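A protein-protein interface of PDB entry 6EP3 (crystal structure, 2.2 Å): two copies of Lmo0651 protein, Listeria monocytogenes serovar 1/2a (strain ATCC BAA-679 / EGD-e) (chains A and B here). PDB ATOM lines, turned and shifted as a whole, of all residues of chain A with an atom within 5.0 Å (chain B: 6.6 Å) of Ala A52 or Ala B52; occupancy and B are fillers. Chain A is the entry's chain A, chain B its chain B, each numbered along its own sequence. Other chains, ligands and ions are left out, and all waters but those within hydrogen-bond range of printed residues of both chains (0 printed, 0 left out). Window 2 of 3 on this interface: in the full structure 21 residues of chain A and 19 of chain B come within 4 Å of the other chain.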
ATOM      1  N   LEU A  47     -28.161  25.870 -28.589  1.00  0.00           N
ATOM      2  CA  LEU A  47     -28.393  24.459 -28.284  1.00  0.00           C
ATOM      3  C   LEU A  47     -27.083  23.712 -28.067  1.00  0.00           C
ATOM      4  O   LEU A  47     -26.929  22.973 -27.086  1.00  0.00           O
ATOM      5  CB  LEU A  47     -29.200  23.805 -29.406  1.00  0.00           C
ATOM      6  CG  LEU A  47     -29.363  22.286 -29.322  1.00  0.00           C
ATOM      7  CD1 LEU A  47     -30.791  21.912 -29.673  1.00  0.00           C
ATOM      8  CD2 LEU A  47     -28.402  21.565 -30.249  1.00  0.00           C
ATOM      9  N   ARG A  48     -26.123  23.890 -28.979  1.00  0.00           N
ATOM     10  CA  ARG A  48     -24.824  23.243 -28.821  1.00  0.00           C
ATOM     11  C   ARG A  48     -24.193  23.612 -27.485  1.00  0.00           C
ATOM     12  O   ARG A  48     -23.690  22.740 -26.764  1.00  0.00           O
ATOM     13  CB  ARG A  48     -23.903  23.615 -29.983  1.00  0.00           C
ATOM     14  CG  ARG A  48     -24.436  23.187 -31.339  1.00  0.00           C
ATOM     15  CD  ARG A  48     -23.320  22.822 -32.304  1.00  0.00           C
ATOM     16  NE  ARG A  48     -23.432  23.551 -33.565  1.00  0.00           N
ATOM     17  CZ  ARG A  48     -24.317  23.274 -34.518  1.00  0.00           C
ATOM     18  NH1 ARG A  48     -24.342  23.996 -35.631  1.00  0.00           N
ATOM     19  NH2 ARG A  48     -25.178  22.275 -34.362  1.00  0.00           N
ATOM     20  N   LYS A  49     -24.230  24.901 -27.129  1.00  0.00           N
ATOM     21  CA  LYS A  49     -23.786  25.319 -25.803  1.00  0.00           C
ATOM     22  C   LYS A  49     -24.437  24.466 -24.728  1.00  0.00           C
ATOM     23  O   LYS A  49     -23.754  23.905 -23.861  1.00  0.00           O
ATOM     24  CB  LYS A  49     -24.102  26.798 -25.575  1.00  0.00           C
ATOM     25  CG  LYS A  49     -22.948  27.738 -25.868  1.00  0.00           C
ATOM     26  CD  LYS A  49     -23.223  29.119 -25.299  1.00  0.00           C
ATOM     27  CE  LYS A  49     -23.634  29.043 -23.835  1.00  0.00           C
ATOM     28  NZ  LYS A  49     -23.320  30.303 -23.104  1.00  0.00           N
ATOM     29  N   ALA A  50     -25.768  24.350 -24.782  1.00  0.00           N
ATOM     30  CA  ALA A  50     -26.481  23.477 -23.858  1.00  0.00           C
ATOM     31  C   ALA A  50     -25.857  22.090 -23.846  1.00  0.00           C
ATOM     32  O   ALA A  50     -25.476  21.573 -22.788  1.00  0.00           O
ATOM     33  CB  ALA A  50     -27.960  23.402 -24.243  1.00  0.00           C
ATOM     34  N   ILE A  51     -25.717  21.485 -25.027  1.00  0.00           N
ATOM     35  CA  ILE A  51     -25.100  20.165 -25.109  1.00  0.00           C
ATOM     36  C   ILE A  51     -23.712  20.208 -24.487  1.00  0.00           C
ATOM     37  O   ILE A  51     -23.346  19.346 -23.676  1.00  0.00           O
ATOM     38  CB  ILE A  51     -25.068  19.676 -26.568  1.00  0.00           C
ATOM     39  CG1 ILE A  51     -26.442  19.129 -26.961  1.00  0.00           C
ATOM     40  CG2 ILE A  51     -24.004  18.604 -26.756  1.00  0.00           C
ATOM     41  CD1 ILE A  51     -26.556  18.740 -28.410  1.00  0.00           C
ATOM     42  N   ALA A  52     -22.935  21.242 -24.828  1.00  0.00           N
ATOM     43  CA  ALA A  52     -21.618  21.419 -24.228  1.00  0.00           C
ATOM     44  C   ALA A  52     -21.722  21.450 -22.712  1.00  0.00           C
ATOM     45  O   ALA A  52     -20.960  20.776 -22.008  1.00  0.00           O
ATOM     46  CB  ALA A  52     -20.962  22.696 -24.757  1.00  0.00           C
ATOM     47  N   THR A  53     -22.680  22.222 -22.191  1.00  0.00           N
ATOM     48  CA  THR A  53     -22.888  22.255 -20.748  1.00  0.00           C
ATOM     49  C   THR A  53     -23.190  20.860 -20.218  1.00  0.00           C
ATOM     50  O   THR A  53     -22.612  20.434 -19.211  1.00  0.00           O
ATOM     51  CB  THR A  53     -24.008  23.236 -20.394  1.00  0.00           C
ATOM     52  OG1 THR A  53     -23.715  24.520 -20.958  1.00  0.00           O
ATOM     53  CG2 THR A  53     -24.134  23.380 -18.883  1.00  0.00           C
ATOM     54  N   LEU A  54     -24.045  20.107 -20.919  1.00  0.00           N
ATOM     55  CA  LEU A  54     -24.352  18.764 -20.447  1.00  0.00           C
ATOM     56  C   LEU A  54     -23.177  17.819 -20.628  1.00  0.00           C
ATOM     57  O   LEU A  54     -23.127  16.783 -19.956  1.00  0.00           O
ATOM     58  CB  LEU A  54     -25.573  18.201 -21.180  1.00  0.00           C
ATOM     59  CG  LEU A  54     -26.881  18.982 -21.110  1.00  0.00           C
ATOM     60  CD1 LEU A  54     -27.772  18.622 -22.283  1.00  0.00           C
ATOM     61  CD2 LEU A  54     -27.581  18.669 -19.802  1.00  0.00           C
ATOM     62  N   THR A  55     -22.210  18.172 -21.478  1.00  0.00           N
ATOM     63  CA  THR A  55     -20.967  17.416 -21.503  1.00  0.00           C
ATOM     64  C   THR A  55     -20.060  17.810 -20.351  1.00  0.00           C
ATOM     65  O   THR A  55     -19.353  16.957 -19.802  1.00  0.00           O
ATOM     66  CB  THR A  55     -20.243  17.614 -22.834  1.00  0.00           C
ATOM     67  OG1 THR A  55     -21.148  17.351 -23.914  1.00  0.00           O
ATOM     68  CG2 THR A  55     -19.055  16.663 -22.934  1.00  0.00           C
ATOM     69  N   ALA A  56     -20.101  19.078 -19.943  1.00  0.00           N
ATOM     70  CA  ALA A  56     -19.300  19.508 -18.807  1.00  0.00           C
ATOM     71  C   ALA A  56     -19.794  18.903 -17.503  1.00  0.00           C
ATOM     72  O   ALA A  56     -19.017  18.797 -16.548  1.00  0.00           O
ATOM     73  CB  ALA A  56     -19.305  21.033 -18.716  1.00  0.00           C
ATOM     74  N   TYR A  62     -19.075  13.299 -25.712  1.00  0.00           N
ATOM     75  CA  TYR A  62     -18.668  13.425 -27.110  1.00  0.00           C
ATOM     76  C   TYR A  62     -17.832  12.200 -27.452  1.00  0.00           C
ATOM     77  O   TYR A  62     -16.621  12.166 -27.226  1.00  0.00           O
ATOM     78  CB  TYR A  62     -17.883  14.711 -27.340  1.00  0.00           C
ATOM     79  CG  TYR A  62     -18.681  15.982 -27.191  1.00  0.00           C
ATOM     80  CD1 TYR A  62     -19.843  16.188 -27.921  1.00  0.00           C
ATOM     81  CD2 TYR A  62     -18.264  16.982 -26.321  1.00  0.00           C
ATOM     82  CE1 TYR A  62     -20.573  17.356 -27.786  1.00  0.00           C
ATOM     83  CE2 TYR A  62     -18.987  18.150 -26.175  1.00  0.00           C
ATOM     84  CZ  TYR A  62     -20.139  18.334 -26.910  1.00  0.00           C
ATOM     85  OH  TYR A  62     -20.858  19.499 -26.766  1.00  0.00           O
ATOM     86  N   LEU B  47     -12.745  22.641 -30.542  1.00  0.00           N
ATOM     87  CA  LEU B  47     -12.156  23.227 -29.342  1.00  0.00           C
ATOM     88  C   LEU B  47     -13.151  23.250 -28.187  1.00  0.00           C
ATOM     89  O   LEU B  47     -12.889  22.698 -27.111  1.00  0.00           O
ATOM     90  CB  LEU B  47     -11.649  24.635 -29.659  1.00  0.00           C
ATOM     91  CG  LEU B  47     -11.183  25.514 -28.500  1.00  0.00           C
ATOM     92  CD1 LEU B  47      -9.895  26.197 -28.882  1.00  0.00           C
ATOM     93  CD2 LEU B  47     -12.247  26.542 -28.145  1.00  0.00           C
ATOM     94  N   ARG B  48     -14.304  23.889 -28.407  1.00  0.00           N
ATOM     95  CA  ARG B  48     -15.384  23.884 -27.426  1.00  0.00           C
ATOM     96  C   ARG B  48     -15.601  22.486 -26.866  1.00  0.00           C
ATOM     97  O   ARG B  48     -15.531  22.270 -25.648  1.00  0.00           O
ATOM     98  CB  ARG B  48     -16.664  24.419 -28.075  1.00  0.00           C
ATOM     99  CG  ARG B  48     -17.956  23.983 -27.405  1.00  0.00           C
ATOM    100  CD  ARG B  48     -19.161  24.675 -28.031  1.00  0.00           C
ATOM    101  NE  ARG B  48     -19.296  26.058 -27.582  1.00  0.00           N
ATOM    102  CZ  ARG B  48     -19.835  27.030 -28.311  1.00  0.00           C
ATOM    103  NH1 ARG B  48     -20.286  26.771 -29.530  1.00  0.00           N
ATOM    104  NH2 ARG B  48     -19.919  28.263 -27.823  1.00  0.00           N
ATOM    105  N   LYS B  49     -15.806  21.514 -27.761  1.00  0.00           N
ATOM    106  CA  LYS B  49     -16.020  20.133 -27.349  1.00  0.00           C
ATOM    107  C   LYS B  49     -14.919  19.676 -26.404  1.00  0.00           C
ATOM    108  O   LYS B  49     -15.189  19.202 -25.291  1.00  0.00           O
ATOM    109  CB  LYS B  49     -16.084  19.234 -28.586  1.00  0.00           C
ATOM    110  CG  LYS B  49     -17.494  18.989 -29.104  1.00  0.00           C
ATOM    111  CD  LYS B  49     -17.541  17.837 -30.096  1.00  0.00           C
ATOM    112  CE  LYS B  49     -17.262  18.306 -31.510  1.00  0.00           C
ATOM    113  NZ  LYS B  49     -17.863  17.383 -32.510  1.00  0.00           N
ATOM    114  N   ALA B  50     -13.663  19.863 -26.820  1.00  0.00           N
ATOM    115  CA  ALA B  50     -12.528  19.520 -25.972  1.00  0.00           C
ATOM    116  C   ALA B  50     -12.684  20.111 -24.578  1.00  0.00           C
ATOM    117  O   ALA B  50     -12.627  19.389 -23.573  1.00  0.00           O
ATOM    118  CB  ALA B  50     -11.230  20.001 -26.623  1.00  0.00           C
ATOM    119  N   ILE B  51     -12.930  21.422 -24.507  1.00  0.00           N
ATOM    120  CA  ILE B  51     -13.075  22.084 -23.213  1.00  0.00           C
ATOM    121  C   ILE B  51     -14.166  21.410 -22.393  1.00  0.00           C
ATOM    122  O   ILE B  51     -13.969  21.086 -21.215  1.00  0.00           O
ATOM    123  CB  ILE B  51     -13.355  23.586 -23.407  1.00  0.00           C
ATOM    124  CG1 ILE B  51     -12.050  24.325 -23.689  1.00  0.00           C
ATOM    125  CG2 ILE B  51     -14.013  24.175 -22.169  1.00  0.00           C
ATOM    126  CD1 ILE B  51     -12.237  25.782 -24.022  1.00  0.00           C
ATOM    127  N   ALA B  52     -15.318  21.147 -23.022  1.00  0.00           N
ATOM    128  CA  ALA B  52     -16.398  20.473 -22.312  1.00  0.00           C
ATOM    129  C   ALA B  52     -15.907  19.163 -21.713  1.00  0.00           C
ATOM    130  O   ALA B  52     -16.110  18.893 -20.523  1.00  0.00           O
ATOM    131  CB  ALA B  52     -17.579  20.234 -23.254  1.00  0.00           C
ATOM    132  N   THR B  53     -15.200  18.364 -22.518  1.00  0.00           N
ATOM    133  CA  THR B  53     -14.666  17.108 -22.012  1.00  0.00           C
ATOM    134  C   THR B  53     -13.742  17.350 -20.827  1.00  0.00           C
ATOM    135  O   THR B  53     -13.861  16.682 -19.792  1.00  0.00           O
ATOM    136  CB  THR B  53     -13.940  16.359 -23.129  1.00  0.00           C
ATOM    137  OG1 THR B  53     -14.829  16.203 -24.243  1.00  0.00           O
ATOM    138  CG2 THR B  53     -13.502  14.984 -22.651  1.00  0.00           C
ATOM    139  N   LEU B  54     -12.859  18.345 -20.929  1.00  0.00           N
ATOM    140  CA  LEU B  54     -11.955  18.601 -19.816  1.00  0.00           C
ATOM    141  C   LEU B  54     -12.661  19.235 -18.628  1.00  0.00           C
ATOM    142  O   LEU B  54     -12.125  19.198 -17.516  1.00  0.00           O
ATOM    143  CB  LEU B  54     -10.789  19.477 -20.263  1.00  0.00           C
ATOM    144  CG  LEU B  54      -9.948  18.917 -21.408  1.00  0.00           C
ATOM    145  CD1 LEU B  54      -9.225  20.025 -22.130  1.00  0.00           C
ATOM    146  CD2 LEU B  54      -8.955  17.928 -20.841  1.00  0.00           C
ATOM    147  N   THR B  55     -13.867  19.773 -18.820  1.00  0.00           N
ATOM    148  CA  THR B  55     -14.659  20.161 -17.660  1.00  0.00           C
ATOM    149  C   THR B  55     -15.297  18.941 -17.011  1.00  0.00           C
ATOM    150  O   THR B  55     -15.470  18.912 -15.788  1.00  0.00           O
ATOM    151  CB  THR B  55     -15.729  21.185 -18.052  1.00  0.00           C
ATOM    152  OG1 THR B  55     -15.123  22.254 -18.787  1.00  0.00           O
ATOM    153  CG2 THR B  55     -16.390  21.765 -16.809  1.00  0.00           C
ATOM    154  N   ALA B  56     -15.631  17.923 -17.810  1.00  0.00           N
ATOM    155  CA  ALA B  56     -16.174  16.689 -17.259  1.00  0.00           C
ATOM    156  C   ALA B  56     -15.137  15.916 -16.457  1.00  0.00           C
ATOM    157  O   ALA B  56     -15.510  15.111 -15.597  1.00  0.00           O
ATOM    158  CB  ALA B  56     -16.729  15.811 -18.380  1.00  0.00           C
ATOM    159  N   GLN B  57     -13.851  16.150 -16.709  1.00  0.00           N
ATOM    160  CA  GLN B  57     -12.775  15.463 -16.011  1.00  0.00           C
ATOM    161  C   GLN B  57     -12.219  16.277 -14.851  1.00  0.00           C
ATOM    162  O   GLN B  57     -11.242  15.858 -14.222  1.00  0.00           O
ATOM    163  CB  GLN B  57     -11.651  15.113 -16.992  1.00  0.00           C
ATOM    164  CG  GLN B  57     -12.091  14.246 -18.163  1.00  0.00           C
ATOM    165  CD  GLN B  57     -11.024  14.112 -19.236  1.00  0.00           C
ATOM    166  OE1 GLN B  57     -10.308  15.066 -19.537  1.00  0.00           O
ATOM    167  NE2 GLN B  57     -10.907  12.920 -19.810  1.00  0.00           N
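O of Lys A49 is in hydrogen-bond range of OG1 of Thr A53 (3.0 Å). The side-chain hydroxyl of Thr B55 is in hydrogen-bond range of the backbone carbonyl oxygen of Ile B51 (2.9 Å). OG1 of Thr A55 is in hydrogen-bond range of O of Ile A51, at 3.0 Å. The backbone NH (N) of Ala A52 sits close to the side-chain hydroxyl (OH) of Tyr A62 (3.3 Å). OG1 of Thr B53 sits at hydrogen-bond distance from O of Lys B49 (3.2 Å).
Among the printed residues, merely in contact across the chains: Lys A49 with Arg B48, Ala A52 with Ala B52, Thr A55 with Ala B52, Thr A55 with Ala B56, Ala A56 with Ala B52, Ala A56 with Thr B55, Ala A56 with Ala B56, Tyr A62 with Lys B49 and Tyr A62 with Ala B52.
Ala A50 touches none of the printed residues of chain B. Ala A52 touches one residue of chain B. Of the printed residues of chain B, Thr A55 touches Ala B52 and Ala B56. Of the printed residues of chain A, Lys B49 touches Tyr A62 (3.4 Å). Ala B50 touches none of the printed residues of chain A. Ala B52 touches four residues of chain A. Printed residues of chain A within 4 Å of Ala B56: Thr A55 and Ala A56. The nearest residue of chain B that does not touch Ala A52 is Arg B48 (4.2 Å).
Printed residues of chain A that touch a printed residue of chain B: Lys A49, Ala A52, Thr A55, Ala A56 and Tyr A62. Hydrophobic or aromatic side chains of chain A within 4 Å of the printed part of chain B: Ala A56 and Tyr A62. Hydrophobic or aromatic side chains of chain B that line the printed part of chain A: Ala B52 and Ala B56. Among the printed residues, 9 pairs touch across the chains.
Lys A49 touches Arg B48, but with the chains exchanged Arg A48 does not touch Lys B49 (7.6 Å). Thr A55 touches Ala B52, but with the chains exchanged Ala A52 does not touch Thr B55 (6.6 Å). Ala A56 touches Ala B52, but with the chains exchanged Ala A52 does not touch Ala B56 (7.4 Å). Ala A56 touches its own counterpart, Ala B56. Of the 9 pairs that touch across the chains among the printed residues, 4 have their exchanged pair printed and touching as well.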
